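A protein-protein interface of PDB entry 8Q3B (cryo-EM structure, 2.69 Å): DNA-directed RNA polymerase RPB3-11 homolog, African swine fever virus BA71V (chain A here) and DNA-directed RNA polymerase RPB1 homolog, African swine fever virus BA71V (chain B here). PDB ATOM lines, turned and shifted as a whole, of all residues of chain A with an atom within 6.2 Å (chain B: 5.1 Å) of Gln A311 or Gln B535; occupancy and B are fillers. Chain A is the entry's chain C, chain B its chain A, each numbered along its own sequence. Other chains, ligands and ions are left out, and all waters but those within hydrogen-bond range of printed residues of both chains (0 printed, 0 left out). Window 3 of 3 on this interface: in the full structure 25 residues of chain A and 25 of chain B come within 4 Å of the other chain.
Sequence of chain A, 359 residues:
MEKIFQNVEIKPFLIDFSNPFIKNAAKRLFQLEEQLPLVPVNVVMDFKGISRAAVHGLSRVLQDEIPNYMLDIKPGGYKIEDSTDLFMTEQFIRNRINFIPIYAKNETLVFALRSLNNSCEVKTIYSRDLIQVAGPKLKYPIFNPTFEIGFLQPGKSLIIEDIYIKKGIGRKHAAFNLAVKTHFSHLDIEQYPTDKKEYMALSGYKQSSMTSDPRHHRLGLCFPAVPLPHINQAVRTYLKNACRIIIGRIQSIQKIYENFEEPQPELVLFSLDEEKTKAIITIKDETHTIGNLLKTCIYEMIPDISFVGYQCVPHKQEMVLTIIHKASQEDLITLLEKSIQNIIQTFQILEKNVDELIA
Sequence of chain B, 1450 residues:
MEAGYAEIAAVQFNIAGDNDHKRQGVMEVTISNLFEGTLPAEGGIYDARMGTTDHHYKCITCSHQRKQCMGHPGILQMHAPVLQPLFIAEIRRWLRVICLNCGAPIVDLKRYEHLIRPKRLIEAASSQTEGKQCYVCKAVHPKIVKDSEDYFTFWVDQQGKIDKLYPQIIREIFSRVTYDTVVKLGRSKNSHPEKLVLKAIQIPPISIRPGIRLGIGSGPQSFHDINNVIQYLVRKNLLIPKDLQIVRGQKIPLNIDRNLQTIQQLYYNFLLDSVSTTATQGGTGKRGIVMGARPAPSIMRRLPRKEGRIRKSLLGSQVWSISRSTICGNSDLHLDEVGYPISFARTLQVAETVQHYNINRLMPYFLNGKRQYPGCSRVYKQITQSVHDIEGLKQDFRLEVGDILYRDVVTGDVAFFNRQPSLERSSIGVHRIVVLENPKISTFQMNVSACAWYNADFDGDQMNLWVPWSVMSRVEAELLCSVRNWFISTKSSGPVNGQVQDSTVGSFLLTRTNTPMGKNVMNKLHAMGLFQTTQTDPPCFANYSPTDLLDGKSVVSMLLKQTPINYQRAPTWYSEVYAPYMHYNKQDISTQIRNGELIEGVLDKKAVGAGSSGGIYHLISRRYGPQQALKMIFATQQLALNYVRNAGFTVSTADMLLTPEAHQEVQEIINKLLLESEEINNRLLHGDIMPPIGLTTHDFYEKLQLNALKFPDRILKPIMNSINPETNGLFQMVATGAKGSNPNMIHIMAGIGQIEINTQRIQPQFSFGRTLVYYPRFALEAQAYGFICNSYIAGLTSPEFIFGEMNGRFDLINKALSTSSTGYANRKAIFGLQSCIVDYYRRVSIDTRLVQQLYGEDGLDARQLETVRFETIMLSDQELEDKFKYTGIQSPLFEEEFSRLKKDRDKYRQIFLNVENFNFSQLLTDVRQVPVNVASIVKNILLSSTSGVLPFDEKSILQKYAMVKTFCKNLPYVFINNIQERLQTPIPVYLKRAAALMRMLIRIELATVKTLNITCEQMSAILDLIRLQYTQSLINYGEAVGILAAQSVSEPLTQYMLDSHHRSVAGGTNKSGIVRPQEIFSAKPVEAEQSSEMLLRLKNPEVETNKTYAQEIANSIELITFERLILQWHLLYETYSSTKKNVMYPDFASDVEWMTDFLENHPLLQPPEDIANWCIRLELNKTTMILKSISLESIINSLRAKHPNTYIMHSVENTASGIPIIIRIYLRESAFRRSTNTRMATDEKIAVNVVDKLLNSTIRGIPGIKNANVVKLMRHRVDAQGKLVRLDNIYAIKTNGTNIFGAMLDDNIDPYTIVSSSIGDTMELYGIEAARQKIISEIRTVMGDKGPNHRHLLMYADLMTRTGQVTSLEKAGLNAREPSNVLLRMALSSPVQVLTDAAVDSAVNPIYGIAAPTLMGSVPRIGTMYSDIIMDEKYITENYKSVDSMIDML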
ATOM      1  N   HIS A 288     -16.239 -14.588  -7.123  1.00  0.00           N
ATOM      2  CA  HIS A 288     -16.258 -13.198  -7.565  1.00  0.00           C
ATOM      3  C   HIS A 288     -16.043 -13.065  -9.064  1.00  0.00           C
ATOM      4  O   HIS A 288     -16.401 -12.033  -9.637  1.00  0.00           O
ATOM      5  CB  HIS A 288     -15.187 -12.393  -6.829  1.00  0.00           C
ATOM      6  CG  HIS A 288     -15.419 -12.279  -5.356  1.00  0.00           C
ATOM      7  ND1 HIS A 288     -15.888 -11.126  -4.765  1.00  0.00           N
ATOM      8  CD2 HIS A 288     -15.243 -13.171  -4.353  1.00  0.00           C
ATOM      9  CE1 HIS A 288     -15.992 -11.312  -3.462  1.00  0.00           C
ATOM     10  NE2 HIS A 288     -15.606 -12.544  -3.185  1.00  0.00           N
ATOM     11  N   GLY A 309     -25.521  -4.775  -8.859  1.00  0.00           N
ATOM     12  CA  GLY A 309     -24.493  -5.110  -7.893  1.00  0.00           C
ATOM     13  C   GLY A 309     -24.478  -6.596  -7.635  1.00  0.00           C
ATOM     14  O   GLY A 309     -25.380  -7.328  -8.042  1.00  0.00           O
ATOM     15  N   TYR A 310     -23.428  -7.041  -6.950  1.00  0.00           N
ATOM     16  CA  TYR A 310     -23.309  -8.444  -6.590  1.00  0.00           C
ATOM     17  C   TYR A 310     -22.612  -8.555  -5.247  1.00  0.00           C
ATOM     18  O   TYR A 310     -21.782  -7.715  -4.887  1.00  0.00           O
ATOM     19  CB  TYR A 310     -22.535  -9.238  -7.647  1.00  0.00           C
ATOM     20  CG  TYR A 310     -21.036  -9.189  -7.475  1.00  0.00           C
ATOM     21  CD1 TYR A 310     -20.317  -8.053  -7.807  1.00  0.00           C
ATOM     22  CD2 TYR A 310     -20.339 -10.285  -6.985  1.00  0.00           C
ATOM     23  CE1 TYR A 310     -18.947  -8.005  -7.653  1.00  0.00           C
ATOM     24  CE2 TYR A 310     -18.969 -10.246  -6.828  1.00  0.00           C
ATOM     25  CZ  TYR A 310     -18.280  -9.104  -7.164  1.00  0.00           C
ATOM     26  OH  TYR A 310     -16.915  -9.059  -7.011  1.00  0.00           O
ATOM     27  N   GLN A 311     -22.962  -9.601  -4.505  1.00  0.00           N
ATOM     28  CA  GLN A 311     -22.320  -9.908  -3.236  1.00  0.00           C
ATOM     29  C   GLN A 311     -22.006 -11.393  -3.184  1.00  0.00           C
ATOM     30  O   GLN A 311     -22.875 -12.228  -3.458  1.00  0.00           O
ATOM     31  CB  GLN A 311     -23.198  -9.512  -2.044  1.00  0.00           C
ATOM     32  CG  GLN A 311     -24.682  -9.732  -2.252  1.00  0.00           C
ATOM     33  CD  GLN A 311     -25.481  -9.498  -0.986  1.00  0.00           C
ATOM     34  OE1 GLN A 311     -24.916  -9.355   0.098  1.00  0.00           O
ATOM     35  NE2 GLN A 311     -26.801  -9.457  -1.118  1.00  0.00           N
ATOM     36  N   CYS A 312     -20.760 -11.713  -2.844  1.00  0.00           N
ATOM     37  CA  CYS A 312     -20.304 -13.082  -2.623  1.00  0.00           C
ATOM     38  C   CYS A 312     -19.818 -13.157  -1.181  1.00  0.00           C
ATOM     39  O   CYS A 312     -18.629 -12.996  -0.898  1.00  0.00           O
ATOM     40  CB  CYS A 312     -19.212 -13.462  -3.618  1.00  0.00           C
ATOM     41  SG  CYS A 312     -19.009 -15.237  -3.857  1.00  0.00           S
ATOM     42  N   VAL A 313     -20.748 -13.399  -0.267  1.00  0.00           N
ATOM     43  CA  VAL A 313     -20.411 -13.413   1.161  1.00  0.00           C
ATOM     44  C   VAL A 313     -19.576 -14.655   1.460  1.00  0.00           C
ATOM     45  O   VAL A 313     -19.968 -15.767   1.068  1.00  0.00           O
ATOM     46  CB  VAL A 313     -21.684 -13.385   2.006  1.00  0.00           C
ATOM     47  CG1 VAL A 313     -21.364 -13.619   3.471  1.00  0.00           C
ATOM     48  CG2 VAL A 313     -22.408 -12.062   1.822  1.00  0.00           C
ATOM     49  N   GLU A 318     -22.196 -18.527  -1.827  1.00  0.00           N
ATOM     50  CA  GLU A 318     -23.059 -18.265  -2.971  1.00  0.00           C
ATOM     51  C   GLU A 318     -22.866 -16.824  -3.413  1.00  0.00           C
ATOM     52  O   GLU A 318     -22.392 -15.977  -2.652  1.00  0.00           O
ATOM     53  CB  GLU A 318     -24.530 -18.531  -2.638  1.00  0.00           C
ATOM     54  CG  GLU A 318     -25.236 -17.363  -1.965  1.00  0.00           C
ATOM     55  CD  GLU A 318     -26.410 -17.795  -1.110  1.00  0.00           C
ATOM     56  OE1 GLU A 318     -26.391 -18.932  -0.594  1.00  0.00           O
ATOM     57  OE2 GLU A 318     -27.353 -16.994  -0.951  1.00  0.00           O
ATOM     58  N   MET A 319     -23.246 -16.560  -4.660  1.00  0.00           N
ATOM     59  CA  MET A 319     -23.182 -15.230  -5.250  1.00  0.00           C
ATOM     60  C   MET A 319     -24.597 -14.756  -5.540  1.00  0.00           C
ATOM     61  O   MET A 319     -25.375 -15.474  -6.179  1.00  0.00           O
ATOM     62  CB  MET A 319     -22.351 -15.243  -6.536  1.00  0.00           C
ATOM     63  CG  MET A 319     -22.292 -13.910  -7.274  1.00  0.00           C
ATOM     64  SD  MET A 319     -22.442 -14.102  -9.059  1.00  0.00           S
ATOM     65  CE  MET A 319     -24.208 -14.333  -9.232  1.00  0.00           C
ATOM     66  N   VAL A 320     -24.925 -13.553  -5.078  1.00  0.00           N
ATOM     67  CA  VAL A 320     -26.235 -12.952  -5.297  1.00  0.00           C
ATOM     68  C   VAL A 320     -26.036 -11.692  -6.125  1.00  0.00           C
ATOM     69  O   VAL A 320     -25.339 -10.765  -5.695  1.00  0.00           O
ATOM     70  CB  VAL A 320     -26.947 -12.630  -3.974  1.00  0.00           C
ATOM     71  CG1 VAL A 320     -28.357 -12.131  -4.240  1.00  0.00           C
ATOM     72  CG2 VAL A 320     -26.974 -13.854  -3.076  1.00  0.00           C
ATOM     73  N   LEU A 321     -26.649 -11.659  -7.306  1.00  0.00           N
ATOM     74  CA  LEU A 321     -26.572 -10.522  -8.216  1.00  0.00           C
ATOM     75  C   LEU A 321     -27.938  -9.854  -8.269  1.00  0.00           C
ATOM     76  O   LEU A 321     -28.941 -10.511  -8.574  1.00  0.00           O
ATOM     77  CB  LEU A 321     -26.132 -10.968  -9.612  1.00  0.00           C
ATOM     78  CG  LEU A 321     -25.990  -9.876 -10.677  1.00  0.00           C
ATOM     79  CD1 LEU A 321     -24.661  -9.163 -10.541  1.00  0.00           C
ATOM     80  CD2 LEU A 321     -26.130 -10.455 -12.072  1.00  0.00           C
ATOM     81  N   THR A 322     -27.973  -8.557  -7.976  1.00  0.00           N
ATOM     82  CA  THR A 322     -29.198  -7.770  -7.949  1.00  0.00           C
ATOM     83  C   THR A 322     -29.161  -6.738  -9.065  1.00  0.00           C
ATOM     84  O   THR A 322     -28.169  -6.012  -9.213  1.00  0.00           O
ATOM     85  CB  THR A 322     -29.369  -7.072  -6.597  1.00  0.00           C
ATOM     86  OG1 THR A 322     -29.294  -8.040  -5.543  1.00  0.00           O
ATOM     87  CG2 THR A 322     -30.706  -6.353  -6.527  1.00  0.00           C
ATOM     88  N   ASP B 332     -19.964  -9.264   7.866  1.00  0.00           N
ATOM     89  CA  ASP B 332     -21.207  -9.471   7.136  1.00  0.00           C
ATOM     90  C   ASP B 332     -22.361  -9.889   8.038  1.00  0.00           C
ATOM     91  O   ASP B 332     -23.431 -10.241   7.531  1.00  0.00           O
ATOM     92  CB  ASP B 332     -20.998 -10.516   6.040  1.00  0.00           C
ATOM     93  CG  ASP B 332     -20.199  -9.978   4.872  1.00  0.00           C
ATOM     94  OD1 ASP B 332     -20.646  -8.995   4.247  1.00  0.00           O
ATOM     95  OD2 ASP B 332     -19.121 -10.537   4.580  1.00  0.00           O
ATOM     96  N   HIS B 334     -25.068  -8.736  10.990  1.00  0.00           N
ATOM     97  CA  HIS B 334     -25.656  -7.563  11.613  1.00  0.00           C
ATOM     98  C   HIS B 334     -25.269  -7.504  13.088  1.00  0.00           C
ATOM     99  O   HIS B 334     -24.828  -8.489  13.683  1.00  0.00           O
ATOM    100  CB  HIS B 334     -27.176  -7.582  11.469  1.00  0.00           C
ATOM    101  CG  HIS B 334     -27.650  -7.444  10.058  1.00  0.00           C
ATOM    102  ND1 HIS B 334     -27.421  -8.407   9.099  1.00  0.00           N
ATOM    103  CD2 HIS B 334     -28.339  -6.455   9.441  1.00  0.00           C
ATOM    104  CE1 HIS B 334     -27.951  -8.018   7.952  1.00  0.00           C
ATOM    105  NE2 HIS B 334     -28.513  -6.837   8.133  1.00  0.00           N
ATOM    106  N   GLN B 532     -23.498  -2.381  -2.401  1.00  0.00           N
ATOM    107  CA  GLN B 532     -23.889  -3.739  -2.763  1.00  0.00           C
ATOM    108  C   GLN B 532     -23.804  -4.723  -1.604  1.00  0.00           C
ATOM    109  O   GLN B 532     -24.276  -5.856  -1.747  1.00  0.00           O
ATOM    110  CB  GLN B 532     -23.027  -4.242  -3.922  1.00  0.00           C
ATOM    111  CG  GLN B 532     -21.591  -4.544  -3.552  1.00  0.00           C
ATOM    112  CD  GLN B 532     -20.704  -4.702  -4.767  1.00  0.00           C
ATOM    113  OE1 GLN B 532     -21.155  -4.554  -5.902  1.00  0.00           O
ATOM    114  NE2 GLN B 532     -19.432  -5.004  -4.537  1.00  0.00           N
ATOM    115  N   THR B 533     -23.225  -4.331  -0.468  1.00  0.00           N
ATOM    116  CA  THR B 533     -23.130  -5.205   0.696  1.00  0.00           C
ATOM    117  C   THR B 533     -23.819  -4.622   1.924  1.00  0.00           C
ATOM    118  O   THR B 533     -23.632  -5.143   3.030  1.00  0.00           O
ATOM    119  CB  THR B 533     -21.664  -5.503   1.024  1.00  0.00           C
ATOM    120  OG1 THR B 533     -20.926  -4.278   1.097  1.00  0.00           O
ATOM    121  CG2 THR B 533     -21.049  -6.400  -0.037  1.00  0.00           C
ATOM    122  N   THR B 534     -24.609  -3.561   1.765  1.00  0.00           N
ATOM    123  CA  THR B 534     -25.270  -2.925   2.896  1.00  0.00           C
ATOM    124  C   THR B 534     -26.501  -3.684   3.374  1.00  0.00           C
ATOM    125  O   THR B 534     -27.038  -3.348   4.435  1.00  0.00           O
ATOM    126  CB  THR B 534     -25.672  -1.494   2.533  1.00  0.00           C
ATOM    127  OG1 THR B 534     -26.398  -1.498   1.298  1.00  0.00           O
ATOM    128  CG2 THR B 534     -24.442  -0.614   2.392  1.00  0.00           C
ATOM    129  N   GLN B 535     -26.959  -4.690   2.630  1.00  0.00           N
ATOM    130  CA  GLN B 535     -28.129  -5.481   3.010  1.00  0.00           C
ATOM    131  C   GLN B 535     -29.377  -4.612   3.147  1.00  0.00           C
ATOM    132  O   GLN B 535     -30.305  -4.948   3.887  1.00  0.00           O
ATOM    133  CB  GLN B 535     -27.872  -6.255   4.308  1.00  0.00           C
ATOM    134  CG  GLN B 535     -27.777  -7.758   4.121  1.00  0.00           C
ATOM    135  CD  GLN B 535     -26.536  -8.175   3.362  1.00  0.00           C
ATOM    136  OE1 GLN B 535     -25.439  -8.213   3.917  1.00  0.00           O
ATOM    137  NE2 GLN B 535     -26.703  -8.491   2.083  1.00  0.00           N
ATOM    138  N   THR B 536     -29.416  -3.496   2.431  1.00  0.00           N
ATOM    139  CA  THR B 536     -30.551  -2.585   2.426  1.00  0.00           C
ATOM    140  C   THR B 536     -31.085  -2.451   1.003  1.00  0.00           C
ATOM    141  O   THR B 536     -30.576  -3.066   0.064  1.00  0.00           O
ATOM    142  CB  THR B 536     -30.156  -1.217   2.994  1.00  0.00           C
ATOM    143  OG1 THR B 536     -31.328  -0.521   3.434  1.00  0.00           O
ATOM    144  CG2 THR B 536     -29.433  -0.381   1.945  1.00  0.00           C
ATOM    145  N   ASP B 537     -32.123  -1.640   0.850  1.00  0.00           N
ATOM    146  CA  ASP B 537     -32.678  -1.380  -0.470  1.00  0.00           C
ATOM    147  C   ASP B 537     -31.747  -0.440  -1.227  1.00  0.00           C
ATOM    148  O   ASP B 537     -31.521   0.686  -0.769  1.00  0.00           O
ATOM    149  CB  ASP B 537     -34.066  -0.766  -0.355  1.00  0.00           C
ATOM    150  CG  ASP B 537     -35.147  -1.804  -0.127  1.00  0.00           C
ATOM    151  OD1 ASP B 537     -35.046  -2.909  -0.701  1.00  0.00           O
ATOM    152  OD2 ASP B 537     -36.099  -1.516   0.626  1.00  0.00           O
ATOM    153  N   LYS B 631     -29.257  -0.983  12.400  1.00  0.00           N
ATOM    154  CA  LYS B 631     -29.235  -1.189  10.956  1.00  0.00           C
ATOM    155  C   LYS B 631     -28.377  -0.135  10.269  1.00  0.00           C
ATOM    156  O   LYS B 631     -27.590  -0.453   9.368  1.00  0.00           O
ATOM    157  CB  LYS B 631     -30.662  -1.172  10.409  1.00  0.00           C
ATOM    158  CG  LYS B 631     -30.772  -1.328   8.896  1.00  0.00           C
ATOM    159  CD  LYS B 631     -30.928  -2.787   8.498  1.00  0.00           C
ATOM    160  CE  LYS B 631     -30.382  -3.058   7.102  1.00  0.00           C
ATOM    161  NZ  LYS B 631     -29.307  -4.084   7.114  1.00  0.00           N
ATOM    162  N   PHE B 634     -24.683  -0.804  10.840  1.00  0.00           N
ATOM    163  CA  PHE B 634     -24.189  -1.839   9.936  1.00  0.00           C
ATOM    164  C   PHE B 634     -24.011  -1.299   8.523  1.00  0.00           C
ATOM    165  O   PHE B 634     -22.990  -1.556   7.873  1.00  0.00           O
ATOM    166  CB  PHE B 634     -25.143  -3.032   9.934  1.00  0.00           C
ATOM    167  CG  PHE B 634     -24.752  -4.115   8.971  1.00  0.00           C
ATOM    168  CD1 PHE B 634     -23.725  -4.991   9.272  1.00  0.00           C
ATOM    169  CD2 PHE B 634     -25.413  -4.257   7.764  1.00  0.00           C
ATOM    170  CE1 PHE B 634     -23.366  -5.986   8.388  1.00  0.00           C
ATOM    171  CE2 PHE B 634     -25.056  -5.251   6.877  1.00  0.00           C
ATOM    172  CZ  PHE B 634     -24.031  -6.115   7.191  1.00  0.00           C
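Among the printed residues, merely in contact across the chains: Gln A311 with Gln B532 (3.8 Å), Gly A309 with Gln B532 (3.9 Å) and Val A313 with Asp B332 (3.97 Å).
Of the printed residues of chain B, Tyr A310 touches Gln B532. Gln A311 touches just these residues of chain B: Gln B532 and Gln B535. Printed residues of chain A within 4 Å of Gln B532: Gly A309 (3.9 Å), Tyr A310 (3.2 Å) and Gln A311 (3.8 Å). Thr B533 touches none of the printed residues of chain A. Printed residues of chain A within 4 Å of Gln B535: Gln A311 (2.8 Å). The nearest residue of chain B that does not touch Gln A311 is Thr B533 (4.3 Å). The nearest residue of chain A that does not touch Gln B535 is Val A313 (5.3 Å). The nearest printed residue of chain B that does not touch Gly A309 is Thr B533 (7.6 Å).
The backbone carbonyl oxygen (O) of Gln B535 is in hydrogen-bond range of the side-chain amino group (NZ) of Lys B631 (3.5 Å). The side-chain hydroxyl (OH) of Tyr A310 lies within hydrogen-bond range of a ring nitrogen (ND1) of His A288 (3.2 Å). The backbone carbonyl oxygen (O) of Gly A309 sits at hydrogen-bond distance from the backbone NH (N) of Thr A322 (2.9 Å). The backbone NH (N) of Gln A311 sits at hydrogen-bond distance from the backbone carbonyl oxygen (O) of Val A320, 2.9 Å away.
Of the 11 printed residues of chain A, 4 touch a printed residue of chain B. Printed residues of chain A that touch a printed residue of chain B: Gly A309, Tyr A310, Gln A311 and Val A313. Of the 10 printed residues of chain B, 3 touch a printed residue of chain A.
The side-chain amide oxygen of Gln B532 sits close to the backbone carbonyl oxygen of Tyr A310 (3.4 Å). NE2 of Gln B535 sits at hydrogen-bond distance from OE1 of Gln A311.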
